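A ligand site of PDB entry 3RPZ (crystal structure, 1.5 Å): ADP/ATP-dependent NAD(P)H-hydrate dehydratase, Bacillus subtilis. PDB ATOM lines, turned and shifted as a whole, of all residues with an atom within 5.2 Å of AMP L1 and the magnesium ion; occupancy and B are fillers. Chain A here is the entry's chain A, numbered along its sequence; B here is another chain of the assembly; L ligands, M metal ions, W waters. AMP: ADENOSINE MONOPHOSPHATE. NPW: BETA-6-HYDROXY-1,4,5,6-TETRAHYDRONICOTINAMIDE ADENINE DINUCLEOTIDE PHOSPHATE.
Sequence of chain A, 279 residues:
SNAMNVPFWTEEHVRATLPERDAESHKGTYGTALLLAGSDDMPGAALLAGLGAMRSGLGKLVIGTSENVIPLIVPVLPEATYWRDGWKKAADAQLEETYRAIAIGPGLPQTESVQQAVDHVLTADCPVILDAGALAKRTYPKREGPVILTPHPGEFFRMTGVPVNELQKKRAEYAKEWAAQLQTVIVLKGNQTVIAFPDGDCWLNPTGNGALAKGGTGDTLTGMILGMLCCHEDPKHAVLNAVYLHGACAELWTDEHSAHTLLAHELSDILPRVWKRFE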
ATOM      1  N   ASP A 131      18.317   4.344 -25.419  1.00  0.00           N
ATOM      2  CA  ASP A 131      18.501   5.782 -25.425  1.00  0.00           C
ATOM      3  C   ASP A 131      19.747   6.143 -26.194  1.00  0.00           C
ATOM      4  O   ASP A 131      20.643   5.313 -26.333  1.00  0.00           O
ATOM      5  CB  ASP A 131      18.620   6.319 -23.970  1.00  0.00           C
ATOM      6  CG  ASP A 131      18.650   7.804 -23.861  1.00  0.00           C
ATOM      7  OD1 ASP A 131      18.041   8.499 -24.699  1.00  0.00           O
ATOM      8  OD2 ASP A 131      19.334   8.281 -22.923  1.00  0.00           O
ATOM      9  N   ALA A 132      19.817   7.384 -26.633  1.00  0.00           N
ATOM     10  CA  ALA A 132      21.115   7.981 -27.015  1.00  0.00           C
ATOM     11  C   ALA A 132      21.852   7.157 -28.076  1.00  0.00           C
ATOM     12  O   ALA A 132      21.305   6.972 -29.148  1.00  0.00           O
ATOM     13  CB  ALA A 132      21.960   8.246 -25.729  1.00  0.00           C
ATOM     14  N   HIS A 152      15.050  12.307 -27.985  1.00  0.00           N
ATOM     15  CA  HIS A 152      14.692  13.689 -28.246  1.00  0.00           C
ATOM     16  C   HIS A 152      14.390  13.850 -29.728  1.00  0.00           C
ATOM     17  O   HIS A 152      14.556  12.908 -30.520  1.00  0.00           O
ATOM     18  CB  HIS A 152      15.758  14.657 -27.726  1.00  0.00           C
ATOM     19  CG  HIS A 152      17.101  14.511 -28.363  1.00  0.00           C
ATOM     20  ND1 HIS A 152      17.324  14.474 -29.735  1.00  0.00           N
ATOM     21  CD2 HIS A 152      18.328  14.488 -27.778  1.00  0.00           C
ATOM     22  CE1 HIS A 152      18.633  14.344 -29.946  1.00  0.00           C
ATOM     23  NE2 HIS A 152      19.268  14.372 -28.778  1.00  0.00           N
ATOM     24  N   GLU A 155      17.002  12.574 -32.253  1.00  0.00           N
ATOM     25  CA  GLU A 155      17.097  11.125 -32.266  1.00  0.00           C
ATOM     26  C   GLU A 155      15.890  10.532 -32.989  1.00  0.00           C
ATOM     27  O   GLU A 155      16.027   9.520 -33.696  1.00  0.00           O
ATOM     28  CB  GLU A 155      17.225  10.576 -30.844  1.00  0.00           C
ATOM     29  CG  GLU A 155      18.613  10.822 -30.279  1.00  0.00           C
ATOM     30  CD  GLU A 155      18.747  10.873 -28.803  1.00  0.00           C
ATOM     31  OE1 GLU A 155      17.756  11.045 -28.063  1.00  0.00           O
ATOM     32  OE2 GLU A 155      19.921  10.813 -28.314  1.00  0.00           O
ATOM     33  N   LYS A 189      10.865  13.225 -26.188  1.00  0.00           N
ATOM     34  CA  LYS A 189      11.189  14.265 -25.230  1.00  0.00           C
ATOM     35  C   LYS A 189      10.995  15.663 -25.809  1.00  0.00           C
ATOM     36  O   LYS A 189      10.811  15.882 -27.010  1.00  0.00           O
ATOM     37  CB  LYS A 189      12.625  13.995 -24.745  1.00  0.00           C
ATOM     38  CG  LYS A 189      12.614  12.821 -23.787  1.00  0.00           C
ATOM     39  CD  LYS A 189      13.665  11.707 -23.868  1.00  0.00           C
ATOM     40  CE  LYS A 189      14.973  12.284 -23.518  1.00  0.00           C
ATOM     41  NZ  LYS A 189      16.226  11.453 -23.831  1.00  0.00           N
ATOM     42  N   GLY A 190      11.031  16.608 -24.862  1.00  0.00           N
ATOM     43  CA  GLY A 190      10.752  18.001 -25.123  1.00  0.00           C
ATOM     44  C   GLY A 190       9.804  18.570 -24.103  1.00  0.00           C
ATOM     45  O   GLY A 190       9.283  17.856 -23.252  1.00  0.00           O
ATOM     46  N   ASN A 191       9.581  19.869 -24.121  1.00  0.00           N
ATOM     47  CA  ASN A 191       8.472  20.428 -23.409  1.00  0.00           C
ATOM     48  C   ASN A 191       7.250  19.573 -23.880  1.00  0.00           C
ATOM     49  O   ASN A 191       7.099  19.206 -25.056  1.00  0.00           O
ATOM     50  CB  ASN A 191       8.328  21.912 -23.789  1.00  0.00           C
ATOM     51  CG  ASN A 191       7.108  22.578 -23.233  1.00  0.00           C
ATOM     52  OD1 ASN A 191       6.817  22.481 -22.078  1.00  0.00           O
ATOM     53  ND2 ASN A 191       6.375  23.294 -24.104  1.00  0.00           N
ATOM     54  N   THR A 193       6.591  16.359 -23.047  1.00  0.00           N
ATOM     55  CA  THR A 193       7.045  15.059 -23.492  1.00  0.00           C
ATOM     56  C   THR A 193       5.829  14.175 -23.811  1.00  0.00           C
ATOM     57  O   THR A 193       4.859  14.128 -23.025  1.00  0.00           O
ATOM     58  CB  THR A 193       7.955  14.406 -22.439  1.00  0.00           C
ATOM     59  OG1 THR A 193       9.231  15.083 -22.442  1.00  0.00           O
ATOM     60  CG2 THR A 193       8.206  12.888 -22.717  1.00  0.00           C
ATOM     61  N   THR A 207       4.978  18.264 -16.537  1.00  0.00           N
ATOM     62  CA  THR A 207       6.019  18.814 -15.687  1.00  0.00           C
ATOM     63  C   THR A 207       7.313  19.113 -16.429  1.00  0.00           C
ATOM     64  O   THR A 207       7.613  18.593 -17.484  1.00  0.00           O
ATOM     65  CB  THR A 207       6.324  17.890 -14.499  1.00  0.00           C
ATOM     66  OG1 THR A 207       6.908  16.698 -14.987  1.00  0.00           O
ATOM     67  CG2 THR A 207       5.121  17.590 -13.652  1.00  0.00           C
ATOM     68  N   GLY A 208       8.132  19.933 -15.792  1.00  0.00           N
ATOM     69  CA  GLY A 208       9.400  20.356 -16.301  1.00  0.00           C
ATOM     70  C   GLY A 208       9.478  21.744 -16.829  1.00  0.00           C
ATOM     71  O   GLY A 208       8.448  22.414 -17.010  1.00  0.00           O
ATOM     72  N   ASN A 209      10.694  22.261 -17.013  1.00  0.00           N
ATOM     73  CA  ASN A 209      10.908  23.609 -17.495  1.00  0.00           C
ATOM     74  C   ASN A 209      12.274  23.728 -18.140  1.00  0.00           C
ATOM     75  O   ASN A 209      12.964  22.670 -18.263  1.00  0.00           O
ATOM     76  CB  ASN A 209      10.710  24.623 -16.387  1.00  0.00           C
ATOM     77  CG  ASN A 209      11.634  24.413 -15.238  1.00  0.00           C
ATOM     78  OD1 ASN A 209      12.805  24.069 -15.450  1.00  0.00           O
ATOM     79  ND2 ASN A 209      11.139  24.550 -13.982  1.00  0.00           N
ATOM     80  N   GLY A 210      12.672  24.920 -18.570  1.00  0.00           N
ATOM     81  CA  GLY A 210      13.919  25.076 -19.278  1.00  0.00           C
ATOM     82  C   GLY A 210      15.169  24.806 -18.442  1.00  0.00           C
ATOM     83  O   GLY A 210      16.271  24.746 -18.984  1.00  0.00           O
ATOM     84  N   LEU A 212      15.821  22.036 -17.495  1.00  0.00           N
ATOM     85  CA  LEU A 212      16.185  20.737 -18.062  1.00  0.00           C
ATOM     86  C   LEU A 212      16.910  20.819 -19.390  1.00  0.00           C
ATOM     87  O   LEU A 212      17.422  19.812 -19.881  1.00  0.00           O
ATOM     88  CB  LEU A 212      14.944  19.829 -18.198  1.00  0.00           C
ATOM     89  CG  LEU A 212      14.280  19.455 -16.895  1.00  0.00           C
ATOM     90  CD1 LEU A 212      12.942  18.783 -17.176  1.00  0.00           C
ATOM     91  CD2 LEU A 212      15.180  18.555 -16.048  1.00  0.00           C
ATOM     92  N   ALA A 213      16.950  22.001 -19.987  1.00  0.00           N
ATOM     93  CA  ALA A 213      17.555  22.208 -21.327  1.00  0.00           C
ATOM     94  C   ALA A 213      19.080  22.365 -21.248  1.00  0.00           C
ATOM     95  O   ALA A 213      19.648  23.415 -21.505  1.00  0.00           O
ATOM     96  CB  ALA A 213      16.904  23.410 -22.009  1.00  0.00           C
ATOM     97  N   LYS A 214      19.703  21.271 -20.784  1.00  0.00           N
ATOM     98  CA  LYS A 214      21.167  21.271 -20.522  1.00  0.00           C
ATOM     99  C   LYS A 214      21.645  19.848 -20.563  1.00  0.00           C
ATOM    100  O   LYS A 214      20.949  18.928 -20.139  1.00  0.00           O
ATOM    101  CB  LYS A 214      21.507  21.950 -19.215  1.00  0.00           C
ATOM    102  CG  LYS A 214      22.997  22.296 -19.055  1.00  0.00           C
ATOM    103  CD  LYS A 214      23.340  22.938 -17.747  1.00  0.00           C
ATOM    104  CE  LYS A 214      22.723  24.317 -17.561  1.00  0.00           C
ATOM    105  NZ  LYS A 214      22.893  24.811 -16.171  1.00  0.00           N
ATOM    106  N   GLY A 216      22.954  16.235 -20.086  1.00  0.00           N
ATOM    107  CA  GLY A 216      22.887  15.258 -19.043  1.00  0.00           C
ATOM    108  C   GLY A 216      21.517  14.929 -18.550  1.00  0.00           C
ATOM    109  O   GLY A 216      21.285  13.896 -17.931  1.00  0.00           O
ATOM    110  N   THR A 217      20.571  15.861 -18.712  1.00  0.00           N
ATOM    111  CA  THR A 217      19.278  15.610 -18.093  1.00  0.00           C
ATOM    112  C   THR A 217      18.554  14.401 -18.674  1.00  0.00           C
ATOM    113  O   THR A 217      17.842  13.692 -17.931  1.00  0.00           O
ATOM    114  CB  THR A 217      18.392  16.845 -18.117  1.00  0.00           C
ATOM    115  OG1 THR A 217      18.157  17.197 -19.474  1.00  0.00           O
ATOM    116  CG2 THR A 217      19.019  18.021 -17.363  1.00  0.00           C
ATOM    117  N   GLY A 218      18.713  14.109 -19.966  1.00  0.00           N
ATOM    118  CA  GLY A 218      18.112  12.932 -20.526  1.00  0.00           C
ATOM    119  C   GLY A 218      18.804  11.649 -20.100  1.00  0.00           C
ATOM    120  O   GLY A 218      18.192  10.593 -20.014  1.00  0.00           O
ATOM    121  N   ASP A 219      20.097  11.763 -19.790  1.00  0.00           N
ATOM    122  CA  ASP A 219      20.846  10.627 -19.252  1.00  0.00           C
ATOM    123  C   ASP A 219      20.306  10.257 -17.881  1.00  0.00           C
ATOM    124  O   ASP A 219      20.081   9.065 -17.565  1.00  0.00           O
ATOM    125  CB  ASP A 219      22.347  10.945 -19.264  1.00  0.00           C
ATOM    126  CG  ASP A 219      22.860  11.360 -20.597  1.00  0.00           C
ATOM    127  OD1 ASP A 219      22.488  10.720 -21.636  1.00  0.00           O
ATOM    128  OD2 ASP A 219      23.633  12.340 -20.663  1.00  0.00           O
ATOM    129  N   LEU A 221      17.249  10.876 -16.845  1.00  0.00           N
ATOM    130  CA  LEU A 221      15.922  10.334 -17.081  1.00  0.00           C
ATOM    131  C   LEU A 221      15.995   8.844 -17.414  1.00  0.00           C
ATOM    132  O   LEU A 221      15.206   8.059 -16.878  1.00  0.00           O
ATOM    133  CB  LEU A 221      15.169  11.101 -18.163  1.00  0.00           C
ATOM    134  CG  LEU A 221      13.845  10.484 -18.537  1.00  0.00           C
ATOM    135  CD1 LEU A 221      12.845  10.550 -17.396  1.00  0.00           C
ATOM    136  CD2 LEU A 221      13.265  11.200 -19.784  1.00  0.00           C
ATOM    137  N   HIS A 246      10.803  13.392 -12.976  1.00  0.00           N
ATOM    138  CA  HIS A 246      11.985  14.075 -13.560  1.00  0.00           C
ATOM    139  C   HIS A 246      11.676  15.542 -13.779  1.00  0.00           C
ATOM    140  O   HIS A 246      12.421  16.415 -13.311  1.00  0.00           O
ATOM    141  CB  HIS A 246      12.367  13.326 -14.807  1.00  0.00           C
ATOM    142  CG  HIS A 246      13.469  13.892 -15.621  1.00  0.00           C
ATOM    143  ND1 HIS A 246      13.230  14.695 -16.738  1.00  0.00           N
ATOM    144  CD2 HIS A 246      14.823  13.752 -15.527  1.00  0.00           C
ATOM    145  CE1 HIS A 246      14.413  14.954 -17.302  1.00  0.00           C
ATOM    146  NE2 HIS A 246      15.383  14.385 -16.600  1.00  0.00           N
ATOM    147  N   ASP B  22      13.394  29.859 -21.873  1.00  0.00           N
ATOM    148  CA  ASP B  22      12.050  29.593 -22.300  1.00  0.00           C
ATOM    149  C   ASP B  22      11.624  28.151 -22.135  1.00  0.00           C
ATOM    150  O   ASP B  22      12.443  27.202 -22.284  1.00  0.00           O
ATOM    151  CB  ASP B  22      11.754  30.004 -23.780  1.00  0.00           C
ATOM    152  CG  ASP B  22      10.265  30.129 -24.081  1.00  0.00           C
ATOM    153  OD1 ASP B  22       9.627  31.106 -23.576  1.00  0.00           O
ATOM    154  OD2 ASP B  22       9.703  29.283 -24.830  1.00  0.00           O
ATOM    155  N   ALA B  23      10.357  27.965 -21.834  1.00  0.00           N
ATOM    156  CA  ALA B  23       9.727  26.677 -21.763  1.00  0.00           C
ATOM    157  C   ALA B  23       9.919  25.884 -23.014  1.00  0.00           C
ATOM    158  O   ALA B  23      10.050  24.678 -22.958  1.00  0.00           O
ATOM    159  CB  ALA B  23       8.189  26.817 -21.524  1.00  0.00           C
ATOM    160  N   GLU B  24       9.951  26.532 -24.158  1.00  0.00           N
ATOM    161  CA  GLU B  24      10.084  25.836 -25.427  1.00  0.00           C
ATOM    162  C   GLU B  24      11.523  26.051 -25.871  1.00  0.00           C
ATOM    163  O   GLU B  24      11.795  26.958 -26.723  1.00  0.00           O
ATOM    164  CB  GLU B  24       9.144  26.431 -26.463  1.00  0.00           C
ATOM    165  CG  GLU B  24       7.701  26.550 -25.938  1.00  0.00           C
ATOM    166  CD  GLU B  24       6.678  26.488 -27.039  1.00  0.00           C
ATOM    167  OE1 GLU B  24       6.941  27.078 -28.123  1.00  0.00           O
ATOM    168  OE2 GLU B  24       5.624  25.850 -26.828  1.00  0.00           O
ATOM    169  N   SER B  25      12.439  25.493 -25.098  1.00  0.00           N
ATOM    170  CA  SER B  25      13.888  25.441 -25.427  1.00  0.00           C
ATOM    171  C   SER B  25      14.375  24.032 -25.120  1.00  0.00           C
ATOM    172  O   SER B  25      13.743  23.247 -24.426  1.00  0.00           O
ATOM    173  CB  SER B  25      14.716  26.467 -24.626  1.00  0.00           C
ATOM    174  OG  SER B  25      14.660  26.223 -23.241  1.00  0.00           O
ATOM    175  N   HIS B  26      15.509  23.705 -25.729  1.00  0.00           N
ATOM    176  CA  HIS B  26      16.254  22.501 -25.422  1.00  0.00           C
ATOM    177  C   HIS B  26      17.710  22.838 -25.300  1.00  0.00           C
ATOM    178  O   HIS B  26      18.098  23.996 -25.556  1.00  0.00           O
ATOM    179  CB  HIS B  26      16.023  21.389 -26.475  1.00  0.00           C
ATOM    180  CG  HIS B  26      16.498  21.771 -27.828  1.00  0.00           C
ATOM    181  ND1 HIS B  26      15.775  22.601 -28.660  1.00  0.00           N
ATOM    182  CD2 HIS B  26      17.607  21.413 -28.521  1.00  0.00           C
ATOM    183  CE1 HIS B  26      16.472  22.767 -29.777  1.00  0.00           C
ATOM    184  NE2 HIS B  26      17.558  22.053 -29.730  1.00  0.00           N
ATOM    185  N   LYS B  27      18.566  21.877 -24.959  1.00  0.00           N
ATOM    186  CA  LYS B  27      19.959  22.238 -24.732  1.00  0.00           C
ATOM    187  C   LYS B  27      20.618  22.901 -25.931  1.00  0.00           C
ATOM    188  O   LYS B  27      21.425  23.801 -25.737  1.00  0.00           O
ATOM    189  CB  LYS B  27      20.764  21.018 -24.211  1.00  0.00           C
ATOM    190  CG  LYS B  27      20.913  19.886 -25.233  1.00  0.00           C
ATOM    191  CD  LYS B  27      21.527  18.659 -24.577  1.00  0.00           C
ATOM    192  CE  LYS B  27      21.783  17.554 -25.556  1.00  0.00           C
ATOM    193  NZ  LYS B  27      20.538  16.983 -26.138  1.00  0.00           N
HETATM  194  P   AMP L   1      18.261  14.885 -23.642  1.00  0.00           P
HETATM  195  O1P AMP L   1      19.361  15.172 -22.557  1.00  0.00           O
HETATM  196  O2P AMP L   1      18.462  15.871 -24.727  1.00  0.00           O
HETATM  197  O3P AMP L   1      18.352  13.417 -23.991  1.00  0.00           O
HETATM  198  O5' AMP L   1      16.980  14.959 -22.814  1.00  0.00           O
HETATM  199  C5' AMP L   1      16.514  16.266 -22.295  1.00  0.00           C
HETATM  200  C4' AMP L   1      15.528  16.042 -21.206  1.00  0.00           C
HETATM  201  O4' AMP L   1      15.167  17.329 -20.603  1.00  0.00           O
HETATM  202  C3' AMP L   1      14.232  15.389 -21.623  1.00  0.00           C
HETATM  203  O3' AMP L   1      13.653  14.741 -20.505  1.00  0.00           O
HETATM  204  C2' AMP L   1      13.450  16.658 -22.004  1.00  0.00           C
HETATM  205  O2' AMP L   1      12.030  16.436 -22.148  1.00  0.00           O
HETATM  206  C1' AMP L   1      13.773  17.576 -20.853  1.00  0.00           C
HETATM  207  N9  AMP L   1      13.713  18.989 -21.225  1.00  0.00           N
HETATM  208  C8  AMP L   1      14.647  19.691 -21.892  1.00  0.00           C
HETATM  209  N7  AMP L   1      14.253  20.991 -22.086  1.00  0.00           N
HETATM  210  C5  AMP L   1      13.042  21.068 -21.495  1.00  0.00           C
HETATM  211  C6  AMP L   1      12.039  22.144 -21.369  1.00  0.00           C
HETATM  212  N6  AMP L   1      12.313  23.362 -21.896  1.00  0.00           N
HETATM  213  N1  AMP L   1      10.914  21.822 -20.724  1.00  0.00           N
HETATM  214  C2  AMP L   1      10.663  20.606 -20.207  1.00  0.00           C
HETATM  215  N3  AMP L   1      11.530  19.549 -20.303  1.00  0.00           N
HETATM  216  C4  AMP L   1      12.627  19.813 -20.950  1.00  0.00           C
HETATM  217  P   NPW L   2      19.632  21.753 -32.877  1.00  0.00           P
HETATM  218  O1  NPW L   2      20.952  21.494 -33.572  1.00  0.00           O
HETATM  219  O2  NPW L   2      19.672  22.344 -31.506  1.00  0.00           O
HETATM  220  O3  NPW L   2      18.601  22.478 -33.755  1.00  0.00           O
HETATM  221  PA  NPW L   2      22.802  14.748 -30.511  1.00  0.00           P
HETATM  222  PB  NPW L   2      23.162  14.663 -27.624  1.00  0.00           P
HETATM  223  C1A NPW L   2      18.440  18.162 -31.901  1.00  0.00           C
HETATM  224  C1B NPW L   2      25.640  11.917 -24.717  1.00  0.00           C
HETATM  225  N1C NPW L   2      25.673  12.876 -23.631  1.00  0.00           N
HETATM  226  N1D NPW L   2      13.977  20.206 -30.477  1.00  0.00           N
HETATM  227  C2A NPW L   2      19.492  19.262 -31.992  1.00  0.00           C
HETATM  228  O2A NPW L   2      18.923  20.310 -32.746  1.00  0.00           O
HETATM  229  C2B NPW L   2      24.268  11.286 -24.967  1.00  0.00           C
HETATM  230  O2B NPW L   2      23.922  10.314 -23.998  1.00  0.00           O
HETATM  231  C2C NPW L   2      26.533  12.860 -22.658  1.00  0.00           C
HETATM  232  C2D NPW L   2      14.638  20.285 -31.636  1.00  0.00           C
HETATM  233  C3A NPW L   2      20.648  18.553 -32.692  1.00  0.00           C
HETATM  234  O3A NPW L   2      20.458  18.480 -34.125  1.00  0.00           O
HETATM  235  C3B NPW L   2      24.552  10.695 -26.364  1.00  0.00           C
HETATM  236  O3B NPW L   2      25.223   9.445 -26.172  1.00  0.00           O
HETATM  237  C3C NPW L   2      26.823  13.670 -21.682  1.00  0.00           C
HETATM  238  N3D NPW L   2      15.817  19.737 -31.971  1.00  0.00           N
HETATM  239  C4B NPW L   2      25.498  11.736 -26.973  1.00  0.00           C
HETATM  240  O4B NPW L   2      25.985  12.590 -25.907  1.00  0.00           O
HETATM  241  C4C NPW L   2      26.034  14.980 -21.664  1.00  0.00           C
HETATM  242  C4D NPW L   2      16.301  18.996 -30.969  1.00  0.00           C
HETATM  243  O4D NPW L   2      19.202  16.959 -31.708  1.00  0.00           O
HETATM  244  C4E NPW L   2      20.536  17.162 -32.109  1.00  0.00           C
HETATM  245  C5A NPW L   2      15.709  18.861 -29.682  1.00  0.00           C
HETATM  246  C5B NPW L   2      24.835  12.620 -28.027  1.00  0.00           C
HETATM  247  O5B NPW L   2      23.580  13.112 -27.546  1.00  0.00           O
HETATM  248  C5C NPW L   2      25.503  15.262 -23.067  1.00  0.00           C
HETATM  249  C5E NPW L   2      21.405  16.979 -30.865  1.00  0.00           C
HETATM  250  O5E NPW L   2      21.458  15.591 -30.547  1.00  0.00           O
HETATM  251  C6C NPW L   2      24.726  14.039 -23.629  1.00  0.00           C
HETATM  252  O6C NPW L   2      23.563  13.714 -22.877  1.00  0.00           O
HETATM  253  C6D NPW L   2      14.453  19.503 -29.424  1.00  0.00           C
HETATM  254  N6D NPW L   2      13.769  19.459 -28.290  1.00  0.00           N
HETATM  255  N7A NPW L   2      16.457  18.098 -28.803  1.00  0.00           N
HETATM  256  C7C NPW L   2      27.737  13.374 -20.618  1.00  0.00           C
HETATM  257  N7C NPW L   2      27.916  14.266 -19.658  1.00  0.00           N
HETATM  258  O7C NPW L   2      28.388  12.297 -20.640  1.00  0.00           O
HETATM  259  C8A NPW L   2      17.567  17.759 -29.571  1.00  0.00           C
HETATM  260  N9A NPW L   2      17.422  18.315 -30.867  1.00  0.00           N
HETATM  261  OA1 NPW L   2      23.757  15.177 -31.548  1.00  0.00           O
HETATM  262  OA2 NPW L   2      22.231  13.420 -30.515  1.00  0.00           O
HETATM  263  OA3 NPW L   2      23.501  15.133 -29.112  1.00  0.00           O
HETATM  264  OB1 NPW L   2      21.739  14.688 -27.310  1.00  0.00           O
HETATM  265  OB2 NPW L   2      24.088  15.502 -26.800  1.00  0.00           O
HETATM  266 MG    MG M   1      19.779  12.177 -24.550  1.00  0.00          MG
HETATM  267  O   HOH W   1      18.493  10.922 -25.482  1.00  0.00           O
HETATM  268  O   HOH W   2      16.913  17.676 -25.909  1.00  0.00           O
HETATM  269  O   HOH W   3      10.463  16.953 -19.920  1.00  0.00           O
HETATM  270  O   HOH W   4      20.179  10.768 -23.096  1.00  0.00           O
HETATM  271  O   HOH W   5      20.756  12.310 -26.264  1.00  0.00           O
HETATM  272  O   HOH W   6      21.125  13.425 -23.664  1.00  0.00           O
HETATM  273  O   HOH W   7      19.399  17.989 -22.280  1.00  0.00           O
HETATM  274  O   HOH W   8      12.926  20.583 -24.920  1.00  0.00           O
HETATM  275  O   HOH W   9       8.569  23.304 -20.290  1.00  0.00           O
HETATM  276  O   HOH W  10      22.168  15.957 -22.716  1.00  0.00           O
HETATM  277  O   HOH W  11      11.037  13.875 -20.532  1.00  0.00           O
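Water W5 lies within hydrogen-bond range of the side-chain carboxylate (OE2) of Glu 155 and an oxygen (OB1) of NPW L2.
Water W6 lies within hydrogen-bond range of O6C of NPW L2 and O1P of AMP L1.
Water W4 bridges the side-chain carboxylate (OD2) of Asp 131 and the side-chain carboxylate (OD1) of Asp 219.
Water W1 lies within hydrogen-bond range of the side-chain carboxylate (OD1) of Asp 131, the side-chain carboxylate (OE1) of Glu 155 and the side-chain amino group (NZ) of Lys 189.
Water W2 bridges an oxygen (O2P) of AMP L1 and a nitrogen (N7A) of NPW L2.
Water W3 lies within hydrogen-bond range of O2' of AMP L1 (2.8 Å) and OG1 of Thr 193 (3.4 Å).
Merely in contact with the magnesium ion: Lys 189.
Of the 27 residues printed, 1 comes within 4 Å of the magnesium ion.
The nearest printed residue that does not touch the magnesium ion is Glu 155 (4.01 Å).
O of Thr 217 lies within hydrogen-bond range of NE2 of His 246 (2.9 Å).
OG of Ser 25 of chain B lies within hydrogen-bond range of O of Asp 22 of chain B, 2.6 Å away.
O of Leu 212 is in hydrogen-bond range of OG1 of Thr 217.
The backbone carbonyl oxygen (O) of Gly 190 sits at hydrogen-bond distance from the side-chain hydroxyl (OG1) of Thr 193, 2.9 Å away.
O of Lys 214 sits at hydrogen-bond distance from OG1 of Thr 217.
The side-chain amino group of Lys 189 lies within salt-bridge range of the side-chain carboxylate of Asp 131 (3.6 Å).
The side-chain carboxylate (OE1) of Glu 155 sits at hydrogen-bond distance from the backbone NH (N) of His 152 (3.0 Å).
The side-chain carboxylate (OD2) of Asp 22 of chain B is in hydrogen-bond range of the backbone NH (N) of Glu 24 of chain B (2.8 Å).
An oxygen (OB1) of NPW L2 is in hydrogen-bond range of a ring nitrogen (NE2) of His 152, at 2.9 Å.
OG1 of Thr 193 sits at hydrogen-bond distance from O2' of AMP L1 (3.1 Å).
NZ of Lys 27 of chain B lies within salt-bridge range of OB1 of NPW L2 (2.8 Å).
O of Ala 23 of chain B is in hydrogen-bond range of N6 of AMP L1.
O2' of AMP L1 is in hydrogen-bond range of N of Gly 190, 2.9 Å away.
An oxygen (O3P) of AMP L1 lies close to the side-chain amino group (NZ) of Lys 189, at 2.9 Å.
An oxygen (O4') of AMP L1 is in hydrogen-bond range of the side-chain hydroxyl (OG1) of Thr 217, 3.2 Å away.
The backbone carbonyl oxygen (O) of Ser 25 of chain B is in hydrogen-bond range of a nitrogen (N6) of AMP L1, at 2.9 Å.
The backbone carbonyl oxygen of Gly 190 sits at hydrogen-bond distance from an oxygen (O2') of AMP L1 (3.3 Å).
The side-chain amino group of Lys 27 of chain B lies within salt-bridge range of an oxygen (O2P) of AMP L1.
O2 of NPW L2 lies within hydrogen-bond range of NE2 of His 26 of chain B (2.8 Å).
N of Gly 218 lies within hydrogen-bond range of O1P of AMP L1 (2.9 Å).
An oxygen (O6C) of NPW L2 sits at hydrogen-bond distance from the side-chain carboxylate of Asp 219 (2.6 Å).
The magnesium ion is bound by an oxygen (O3P) of AMP L1 (2.0 Å), water W5 (2.0 Å), water W1 (2.0 Å), water W6 (2.0 Å) and water W4 (2.1 Å).
The magnesium ion has five donor atoms within binding distance.
The backbone carbonyl oxygen (O) of Asn 209 sits close to a nitrogen (N1) of AMP L1 (3.3 Å).
O of Leu 212 lies close to O4' of AMP L1 (3.4 Å).
His 152 touches AMP L1 (CD2 to O2P, 3.4 Å).
CA of Asn 191 touches C2 of AMP L1, at 3.9 Å.
C of Gly 208 touches C2 of AMP L1, at 3.8 Å.
CA of Gly 210 touches N6 of AMP L1, at 3.5 Å.
N of Ala 213 touches N7 of AMP L1 (3.6 Å).
CD2 of Leu 221 touches O3' of AMP L1, at 3.6 Å.
His 246 touches AMP L1.
Asp 22 of chain B touches AMP L1 (O to N6, 3.9 Å).
Within 4 Å of AMP L1: His 152, Lys 189, Gly 190, Asn 191, Thr 193, Gly 208, Asn 209, Gly 210, Leu 212, Ala 213, Thr 217, Gly 218, Leu 221, His 246, Asp 22 of chain B, Ala 23 of chain B, Ser 25 of chain B and Lys 27 of chain B.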
